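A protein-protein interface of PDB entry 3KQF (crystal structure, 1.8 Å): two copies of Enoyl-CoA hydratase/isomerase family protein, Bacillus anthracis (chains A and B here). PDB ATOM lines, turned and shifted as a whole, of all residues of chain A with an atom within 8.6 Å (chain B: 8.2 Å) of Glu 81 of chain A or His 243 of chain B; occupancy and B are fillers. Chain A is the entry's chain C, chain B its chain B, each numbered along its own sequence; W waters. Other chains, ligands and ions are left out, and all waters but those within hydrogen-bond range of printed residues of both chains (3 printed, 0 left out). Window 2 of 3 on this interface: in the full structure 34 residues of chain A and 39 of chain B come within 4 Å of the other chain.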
ATOM      1  N   ARG A  76       7.382   1.624   2.725  1.00  0.00           N
ATOM      2  CA  ARG A  76       6.534   2.795   2.908  1.00  0.00           C
ATOM      3  C   ARG A  76       6.545   3.266   4.368  1.00  0.00           C
ATOM      4  O   ARG A  76       6.548   4.467   4.633  1.00  0.00           O
ATOM      5  CB  ARG A  76       5.099   2.489   2.461  1.00  0.00           C
ATOM      6  CG  ARG A  76       4.175   3.709   2.447  1.00  0.00           C
ATOM      7  CD  ARG A  76       4.644   4.759   1.442  1.00  0.00           C
ATOM      8  NE  ARG A  76       4.694   4.228   0.079  1.00  0.00           N
ATOM      9  CZ  ARG A  76       3.667   4.193  -0.771  1.00  0.00           C
ATOM     10  NH1 ARG A  76       2.462   4.646  -0.419  1.00  0.00           N
ATOM     11  NH2 ARG A  76       3.842   3.694  -1.985  1.00  0.00           N
ATOM     12  N   GLY A  78       8.891   3.354   6.433  1.00  0.00           N
ATOM     13  CA  GLY A  78      10.110   4.106   6.764  1.00  0.00           C
ATOM     14  C   GLY A  78      10.325   5.385   5.968  1.00  0.00           C
ATOM     15  O   GLY A  78      11.384   6.003   6.042  1.00  0.00           O
ATOM     16  N   MET A  79       9.316   5.789   5.210  1.00  0.00           N
ATOM     17  CA  MET A  79       9.410   6.980   4.393  1.00  0.00           C
ATOM     18  C   MET A  79       8.776   8.219   5.020  1.00  0.00           C
ATOM     19  O   MET A  79       7.687   8.158   5.584  1.00  0.00           O
ATOM     20  CB  MET A  79       8.722   6.724   3.048  1.00  0.00           C
ATOM     21  CG  MET A  79       9.462   5.793   2.154  1.00  0.00           C
ATOM     22  SD  MET A  79       8.486   5.632   0.498  1.00  0.00           S
ATOM     23  CE  MET A  79       9.952   4.963  -0.587  1.00  0.00           C
ATOM     24  N   ASN A  80       9.462   9.344   4.912  1.00  0.00           N
ATOM     25  CA  ASN A  80       8.894  10.602   5.386  1.00  0.00           C
ATOM     26  C   ASN A  80       7.922  11.086   4.308  1.00  0.00           C
ATOM     27  O   ASN A  80       7.797  10.453   3.264  1.00  0.00           O
ATOM     28  CB  ASN A  80       9.975  11.628   5.735  1.00  0.00           C
ATOM     29  CG  ASN A  80      10.900  11.949   4.575  1.00  0.00           C
ATOM     30  OD1 ASN A  80      10.507  11.921   3.418  1.00  0.00           O
ATOM     31  ND2 ASN A  80      12.140  12.289   4.898  1.00  0.00           N
ATOM     32  N   GLU A  81       7.227  12.190   4.546  1.00  0.00           N
ATOM     33  CA  GLU A  81       6.239  12.672   3.572  1.00  0.00           C
ATOM     34  C   GLU A  81       6.814  12.902   2.173  1.00  0.00           C
ATOM     35  O   GLU A  81       6.197  12.515   1.176  1.00  0.00           O
ATOM     36  CB  GLU A  81       5.538  13.926   4.100  1.00  0.00           C
ATOM     37  CG  GLU A  81       4.636  13.619   5.293  1.00  0.00           C
ATOM     38  CD  GLU A  81       4.067  14.848   5.946  1.00  0.00           C
ATOM     39  OE1 GLU A  81       4.565  15.962   5.675  1.00  0.00           O
ATOM     40  OE2 GLU A  81       3.131  14.702   6.760  1.00  0.00           O
ATOM     41  N   GLU A  82       7.992  13.517   2.107  1.00  0.00           N
ATOM     42  CA  GLU A  82       8.644  13.803   0.832  1.00  0.00           C
ATOM     43  C   GLU A  82       8.925  12.522   0.035  1.00  0.00           C
ATOM     44  O   GLU A  82       8.662  12.452  -1.169  1.00  0.00           O
ATOM     45  CB  GLU A  82       9.938  14.568   1.089  1.00  0.00           C
ATOM     46  CG  GLU A  82      10.655  15.043  -0.149  1.00  0.00           C
ATOM     47  CD  GLU A  82      11.823  15.950   0.179  1.00  0.00           C
ATOM     48  OE1 GLU A  82      12.167  16.087   1.378  1.00  0.00           O
ATOM     49  OE2 GLU A  82      12.392  16.541  -0.764  1.00  0.00           O
ATOM     50  N   GLN A  83       9.469  11.517   0.715  1.00  0.00           N
ATOM     51  CA  GLN A  83       9.760  10.226   0.090  1.00  0.00           C
ATOM     52  C   GLN A  83       8.480   9.515  -0.306  1.00  0.00           C
ATOM     53  O   GLN A  83       8.432   8.843  -1.345  1.00  0.00           O
ATOM     54  CB  GLN A  83      10.578   9.360   1.045  1.00  0.00           C
ATOM     55  CG  GLN A  83      11.987   9.900   1.269  1.00  0.00           C
ATOM     56  CD  GLN A  83      12.649   9.333   2.513  1.00  0.00           C
ATOM     57  OE1 GLN A  83      12.002   9.165   3.553  1.00  0.00           O
ATOM     58  NE2 GLN A  83      13.955   9.088   2.433  1.00  0.00           N
ATOM     59  N   VAL A  84       7.434   9.646   0.509  1.00  0.00           N
ATOM     60  CA  VAL A  84       6.152   9.026   0.151  1.00  0.00           C
ATOM     61  C   VAL A  84       5.684   9.613  -1.182  1.00  0.00           C
ATOM     62  O   VAL A  84       5.273   8.869  -2.080  1.00  0.00           O
ATOM     63  CB  VAL A  84       5.062   9.214   1.221  1.00  0.00           C
ATOM     64  CG1 VAL A  84       3.729   8.630   0.731  1.00  0.00           C
ATOM     65  CG2 VAL A  84       5.468   8.560   2.514  1.00  0.00           C
ATOM     66  N   ARG A  85       5.744  10.939  -1.310  1.00  0.00           N
ATOM     67  CA  ARG A  85       5.359  11.600  -2.561  1.00  0.00           C
ATOM     68  C   ARG A  85       6.202  11.106  -3.736  1.00  0.00           C
ATOM     69  O   ARG A  85       5.664  10.816  -4.801  1.00  0.00           O
ATOM     70  CB  ARG A  85       5.442  13.125  -2.461  1.00  0.00           C
ATOM     71  CG  ARG A  85       4.255  13.762  -1.748  1.00  0.00           C
ATOM     72  CD  ARG A  85       4.274  15.295  -1.865  1.00  0.00           C
ATOM     73  NE  ARG A  85       5.318  15.899  -1.044  1.00  0.00           N
ATOM     74  CZ  ARG A  85       5.149  16.324   0.208  1.00  0.00           C
ATOM     75  NH1 ARG A  85       3.962  16.231   0.804  1.00  0.00           N
ATOM     76  NH2 ARG A  85       6.175  16.855   0.867  1.00  0.00           N
ATOM     77  N   HIS A  86       7.518  11.014  -3.556  1.00  0.00           N
ATOM     78  CA  HIS A  86       8.360  10.519  -4.644  1.00  0.00           C
ATOM     79  C   HIS A  86       8.005   9.080  -5.029  1.00  0.00           C
ATOM     80  O   HIS A  86       7.910   8.763  -6.213  1.00  0.00           O
ATOM     81  CB  HIS A  86       9.847  10.603  -4.312  1.00  0.00           C
ATOM     82  CG  HIS A  86      10.718   9.922  -5.324  1.00  0.00           C
ATOM     83  ND1 HIS A  86      10.999  10.473  -6.558  1.00  0.00           N
ATOM     84  CD2 HIS A  86      11.360   8.729  -5.290  1.00  0.00           C
ATOM     85  CE1 HIS A  86      11.778   9.651  -7.238  1.00  0.00           C
ATOM     86  NE2 HIS A  86      12.019   8.590  -6.487  1.00  0.00           N
ATOM     87  N   ALA A  87       7.807   8.218  -4.035  1.00  0.00           N
ATOM     88  CA  ALA A  87       7.474   6.815  -4.288  1.00  0.00           C
ATOM     89  C   ALA A  87       6.115   6.673  -4.993  1.00  0.00           C
ATOM     90  O   ALA A  87       5.981   5.873  -5.922  1.00  0.00           O
ATOM     91  CB  ALA A  87       7.499   6.007  -2.987  1.00  0.00           C
ATOM     92  N   VAL A  88       5.116   7.453  -4.576  1.00  0.00           N
ATOM     93  CA  VAL A  88       3.801   7.376  -5.230  1.00  0.00           C
ATOM     94  C   VAL A  88       3.906   7.889  -6.660  1.00  0.00           C
ATOM     95  O   VAL A  88       3.232   7.376  -7.546  1.00  0.00           O
ATOM     96  CB  VAL A  88       2.678   8.108  -4.443  1.00  0.00           C
ATOM     97  CG1 VAL A  88       1.388   8.108  -5.224  1.00  0.00           C
ATOM     98  CG2 VAL A  88       2.453   7.426  -3.082  1.00  0.00           C
ATOM     99  N   ALA A 143      -6.475   3.696   5.806  1.00  0.00           N
ATOM    100  CA  ALA A 143      -6.682   5.138   5.847  1.00  0.00           C
ATOM    101  C   ALA A 143      -5.933   5.885   4.739  1.00  0.00           C
ATOM    102  O   ALA A 143      -5.584   7.040   4.915  1.00  0.00           O
ATOM    103  CB  ALA A 143      -6.342   5.721   7.230  1.00  0.00           C
ATOM    104  N   ILE A 144      -5.701   5.227   3.602  1.00  0.00           N
ATOM    105  CA  ILE A 144      -5.168   5.918   2.429  1.00  0.00           C
ATOM    106  C   ILE A 144      -6.153   5.628   1.287  1.00  0.00           C
ATOM    107  O   ILE A 144      -7.216   5.015   1.508  1.00  0.00           O
ATOM    108  CB  ILE A 144      -3.684   5.544   2.095  1.00  0.00           C
ATOM    109  CG1 ILE A 144      -3.550   4.071   1.689  1.00  0.00           C
ATOM    110  CG2 ILE A 144      -2.785   5.873   3.280  1.00  0.00           C
ATOM    111  CD1 ILE A 144      -2.153   3.684   1.257  1.00  0.00           C
ATOM    112  N   ILE B 210     -11.302  10.162   6.484  1.00  0.00           N
ATOM    113  CA  ILE B 210     -10.759  11.140   5.537  1.00  0.00           C
ATOM    114  C   ILE B 210     -10.529  10.449   4.190  1.00  0.00           C
ATOM    115  O   ILE B 210     -10.828  10.992   3.126  1.00  0.00           O
ATOM    116  CB  ILE B 210      -9.435  11.744   6.049  1.00  0.00           C
ATOM    117  CG1 ILE B 210      -9.658  12.492   7.357  1.00  0.00           C
ATOM    118  CG2 ILE B 210      -8.828  12.687   4.997  1.00  0.00           C
ATOM    119  CD1 ILE B 210      -8.338  12.900   8.064  1.00  0.00           C
ATOM    120  N   TYR B 238      -4.850  12.288  -3.029  1.00  0.00           N
ATOM    121  CA  TYR B 238      -3.880  11.509  -2.241  1.00  0.00           C
ATOM    122  C   TYR B 238      -3.111  12.419  -1.279  1.00  0.00           C
ATOM    123  O   TYR B 238      -2.769  12.003  -0.177  1.00  0.00           O
ATOM    124  CB  TYR B 238      -2.913  10.730  -3.145  1.00  0.00           C
ATOM    125  CG  TYR B 238      -2.186   9.628  -2.397  1.00  0.00           C
ATOM    126  CD1 TYR B 238      -2.757   8.374  -2.290  1.00  0.00           C
ATOM    127  CD2 TYR B 238      -0.951   9.836  -1.783  1.00  0.00           C
ATOM    128  CE1 TYR B 238      -2.150   7.357  -1.613  1.00  0.00           C
ATOM    129  CE2 TYR B 238      -0.315   8.783  -1.074  1.00  0.00           C
ATOM    130  CZ  TYR B 238      -0.955   7.549  -0.992  1.00  0.00           C
ATOM    131  OH  TYR B 238      -0.412   6.458  -0.334  1.00  0.00           O
ATOM    132  N   GLU B 239      -2.848  13.667  -1.688  1.00  0.00           N
ATOM    133  CA  GLU B 239      -2.165  14.628  -0.810  1.00  0.00           C
ATOM    134  C   GLU B 239      -2.948  14.863   0.480  1.00  0.00           C
ATOM    135  O   GLU B 239      -2.360  15.200   1.503  1.00  0.00           O
ATOM    136  CB  GLU B 239      -1.918  15.962  -1.526  1.00  0.00           C
ATOM    137  CG  GLU B 239      -0.898  15.875  -2.648  1.00  0.00           C
ATOM    138  CD  GLU B 239       0.533  15.721  -2.158  1.00  0.00           C
ATOM    139  OE1 GLU B 239       1.408  15.489  -3.012  1.00  0.00           O
ATOM    140  OE2 GLU B 239       0.791  15.852  -0.937  1.00  0.00           O
ATOM    141  N   GLY B 240      -4.266  14.663   0.425  1.00  0.00           N
ATOM    142  CA  GLY B 240      -5.141  14.812   1.570  1.00  0.00           C
ATOM    143  C   GLY B 240      -5.040  13.704   2.612  1.00  0.00           C
ATOM    144  O   GLY B 240      -5.579  13.853   3.720  1.00  0.00           O
ATOM    145  N   VAL B 241      -4.430  12.567   2.259  1.00  0.00           N
ATOM    146  CA  VAL B 241      -4.237  11.486   3.236  1.00  0.00           C
ATOM    147  C   VAL B 241      -2.792  11.413   3.720  1.00  0.00           C
ATOM    148  O   VAL B 241      -2.536  10.941   4.812  1.00  0.00           O
ATOM    149  CB  VAL B 241      -4.640  10.061   2.717  1.00  0.00           C
ATOM    150  CG1 VAL B 241      -6.094  10.018   2.321  1.00  0.00           C
ATOM    151  CG2 VAL B 241      -3.733   9.591   1.569  1.00  0.00           C
ATOM    152  N   ILE B 242      -1.848  11.896   2.920  1.00  0.00           N
ATOM    153  CA  ILE B 242      -0.430  11.813   3.285  1.00  0.00           C
ATOM    154  C   ILE B 242      -0.025  12.362   4.660  1.00  0.00           C
ATOM    155  O   ILE B 242       0.783  11.732   5.342  1.00  0.00           O
ATOM    156  CB  ILE B 242       0.480  12.498   2.231  1.00  0.00           C
ATOM    157  CG1 ILE B 242       0.586  11.620   0.990  1.00  0.00           C
ATOM    158  CG2 ILE B 242       1.872  12.721   2.795  1.00  0.00           C
ATOM    159  CD1 ILE B 242       1.466  12.219  -0.114  1.00  0.00           C
ATOM    160  N   HIS B 243      -0.547  13.521   5.056  1.00  0.00           N
ATOM    161  CA  HIS B 243      -0.141  14.145   6.340  1.00  0.00           C
ATOM    162  C   HIS B 243      -1.039  13.786   7.520  1.00  0.00           C
ATOM    163  O   HIS B 243      -0.829  14.297   8.628  1.00  0.00           O
ATOM    164  CB  HIS B 243      -0.109  15.685   6.230  1.00  0.00           C
ATOM    165  CG  HIS B 243       0.739  16.218   5.111  1.00  0.00           C
ATOM    166  ND1 HIS B 243       2.006  16.722   5.312  1.00  0.00           N
ATOM    167  CD2 HIS B 243       0.480  16.376   3.791  1.00  0.00           C
ATOM    168  CE1 HIS B 243       2.500  17.144   4.161  1.00  0.00           C
ATOM    169  NE2 HIS B 243       1.594  16.948   3.223  1.00  0.00           N
ATOM    170  N   THR B 244      -2.005  12.893   7.310  1.00  0.00           N
ATOM    171  CA  THR B 244      -2.962  12.523   8.353  1.00  0.00           C
ATOM    172  C   THR B 244      -2.406  11.559   9.397  1.00  0.00           C
ATOM    173  O   THR B 244      -1.577  10.689   9.089  1.00  0.00           O
ATOM    174  CB  THR B 244      -4.256  11.872   7.754  1.00  0.00           C
ATOM    175  OG1 THR B 244      -3.947  10.608   7.139  1.00  0.00           O
ATOM    176  CG2 THR B 244      -4.931  12.800   6.733  1.00  0.00           C
ATOM    177  N   LYS B 245      -2.876  11.718  10.634  1.00  0.00           N
ATOM    178  CA  LYS B 245      -2.510  10.815  11.711  1.00  0.00           C
ATOM    179  C   LYS B 245      -3.142   9.433  11.464  1.00  0.00           C
ATOM    180  O   LYS B 245      -2.560   8.410  11.836  1.00  0.00           O
ATOM    181  CB  LYS B 245      -2.972  11.322  13.089  1.00  0.00           C
ATOM    182  CG  LYS B 245      -2.237  12.515  13.711  1.00  0.00           C
ATOM    183  CD  LYS B 245      -2.825  13.879  13.353  1.00  0.00           C
ATOM    184  CE  LYS B 245      -2.311  14.944  14.338  1.00  0.00           C
ATOM    185  NZ  LYS B 245      -3.019  16.255  14.220  1.00  0.00           N
ATOM    186  N   ASP B 246      -4.335   9.414  10.853  1.00  0.00           N
ATOM    187  CA  ASP B 246      -5.030   8.154  10.533  1.00  0.00           C
ATOM    188  C   ASP B 246      -4.149   7.260   9.647  1.00  0.00           C
ATOM    189  O   ASP B 246      -4.075   6.058   9.865  1.00  0.00           O
ATOM    190  CB  ASP B 246      -6.410   8.386   9.869  1.00  0.00           C
ATOM    191  CG  ASP B 246      -7.528   8.812  10.883  1.00  0.00           C
ATOM    192  OD1 ASP B 246      -7.337   8.732  12.116  1.00  0.00           O
ATOM    193  OD2 ASP B 246      -8.621   9.204  10.430  1.00  0.00           O
ATOM    194  N   ARG B 247      -3.477   7.853   8.656  1.00  0.00           N
ATOM    195  CA  ARG B 247      -2.570   7.102   7.788  1.00  0.00           C
ATOM    196  C   ARG B 247      -1.481   6.405   8.611  1.00  0.00           C
ATOM    197  O   ARG B 247      -1.112   5.256   8.340  1.00  0.00           O
ATOM    198  CB  ARG B 247      -1.929   8.033   6.749  1.00  0.00           C
ATOM    199  CG  ARG B 247      -0.845   7.377   5.939  1.00  0.00           C
ATOM    200  CD  ARG B 247      -0.157   8.343   4.986  1.00  0.00           C
ATOM    201  NE  ARG B 247       1.043   7.713   4.466  1.00  0.00           N
ATOM    202  CZ  ARG B 247       2.263   7.847   4.988  1.00  0.00           C
ATOM    203  NH1 ARG B 247       3.270   7.186   4.446  1.00  0.00           N
ATOM    204  NH2 ARG B 247       2.487   8.635   6.039  1.00  0.00           N
ATOM    205  N   LEU B 248      -0.942   7.113   9.603  1.00  0.00           N
ATOM    206  CA  LEU B 248       0.092   6.537  10.459  1.00  0.00           C
ATOM    207  C   LEU B 248      -0.522   5.425  11.312  1.00  0.00           C
ATOM    208  O   LEU B 248       0.081   4.366  11.478  1.00  0.00           O
ATOM    209  CB  LEU B 248       0.753   7.602  11.343  1.00  0.00           C
ATOM    210  CG  LEU B 248       1.508   8.712  10.611  1.00  0.00           C
ATOM    211  CD1 LEU B 248       2.076   9.733  11.591  1.00  0.00           C
ATOM    212  CD2 LEU B 248       2.605   8.108   9.746  1.00  0.00           C
ATOM    213  N   GLU B 265      -8.432  12.531  11.467  1.00  0.00           N
ATOM    214  CA  GLU B 265      -7.300  13.449  11.570  1.00  0.00           C
ATOM    215  C   GLU B 265      -6.062  12.821  10.948  1.00  0.00           C
ATOM    216  O   GLU B 265      -5.092  13.528  10.653  1.00  0.00           O
ATOM    217  CB  GLU B 265      -7.004  13.809  13.032  1.00  0.00           C
ATOM    218  CG  GLU B 265      -7.960  14.799  13.650  1.00  0.00           C
ATOM    219  CD  GLU B 265      -7.547  15.182  15.056  1.00  0.00           C
ATOM    220  OE1 GLU B 265      -7.122  16.343  15.247  1.00  0.00           O
ATOM    221  OE2 GLU B 265      -7.573  14.308  15.951  1.00  0.00           O
ATOM    222  OXT GLU B 265      -5.995  11.606  10.763  1.00  0.00           O
HETATM  223  O   HOH W   1       1.239   6.028   2.032  1.00  0.00           O
HETATM  224  O   HOH W   2       5.308   9.523   6.692  1.00  0.00           O
HETATM  225  O   HOH W   3      -6.445   9.261   6.369  1.00  0.00           O
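The side-chain hydroxyl (OH) of Tyr 238 of chain B sits at hydrogen-bond distance from the guanidinium group (NH1) of Arg 76 of chain A (3.4 Å). NH1 of Arg 85 of chain A lies within salt-bridge range of OE2 of Glu 239 of chain B (3.6 Å). OE1 of Glu 81 of chain A is in hydrogen-bond range of ND1 of His 243 of chain B, 2.7 Å away. A ring nitrogen (NE2) of His 243 of chain B is in hydrogen-bond range of the guanidinium group (NH1) of Arg 85 of chain A, 3.5 Å away.
OG1 of Thr 244 of chain B is in hydrogen-bond range of O of Val 241 of chain B. OG1 of Thr 244 of chain B lies within hydrogen-bond range of N of Arg 247 of chain B (3.2 Å). The chain-end carboxylate of Glu 265 of chain B lies within hydrogen-bond range of the backbone NH of Asp 246 of chain B (2.8 Å).
Among the printed residues, pairs that only touch across the chains: Val 84 of chain A with Arg 247 of chain B, Ala 143 of chain A with Asp 246 of chain B, Arg 85 of chain A with Ile 242 of chain B, Ile 144 of chain A with Arg 247 of chain B, Ile 144 of chain A with Tyr 238 of chain B, Val 88 of chain A with Tyr 238 of chain B, Glu 81 of chain A with Ile 242 of chain B, Ala 143 of chain A with Arg 247 of chain B and Ala 143 of chain A with Val 241 of chain B.
Glu 81 of chain A touches just these residues of chain B: Ile 242 and His 243. His 243 of chain B touches just these residues of chain A: Glu 81 (2.7 Å) and Arg 85 (3.5 Å). Printed residues of chain B within 4 Å of Val 84 of chain A: Arg 247. Printed residues of chain B within 4 Å of Ala 143 of chain A: Val 241, Asp 246 and Arg 247. Of the printed residues of chain A, Ile 242 of chain B touches Glu 81 and Arg 85. His 86 of chain A touches none of the printed residues of chain B. The nearest printed residue of chain B that does not touch Glu 81 of chain A is Thr 244 of chain B (5.5 Å). The nearest residue of chain A that does not touch His 243 of chain B is Glu 82 of chain A (6.9 Å).
Along chain A the printed residues that touch a printed residue of chain B span positions 76 to 144. Among the printed residues, 13 pairs touch across the chains.
No position is printed for both chains. Of the 13 pairs that touch across the chains among the printed residues, none has its exchanged pair printed and touching as well.
Water W3 lies within hydrogen-bond range of O of Ala 143 of chain A (2.8 Å) and OG1 of Thr 244 of chain B (2.9 Å). Water W1 lies within hydrogen-bond range of the side-chain hydroxyl of Tyr 238 of chain B (2.9 Å), the guanidinium group of Arg 247 of chain B (3.0 Å) and the guanidinium group of Arg 76 of chain A (3.1 Å). Water W2 lies within hydrogen-bond range of the backbone carbonyl oxygen (O) of Met 79 of chain A (3.0 Å) and the guanidinium group (NH2) of Arg 247 of chain B (3.0 Å).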
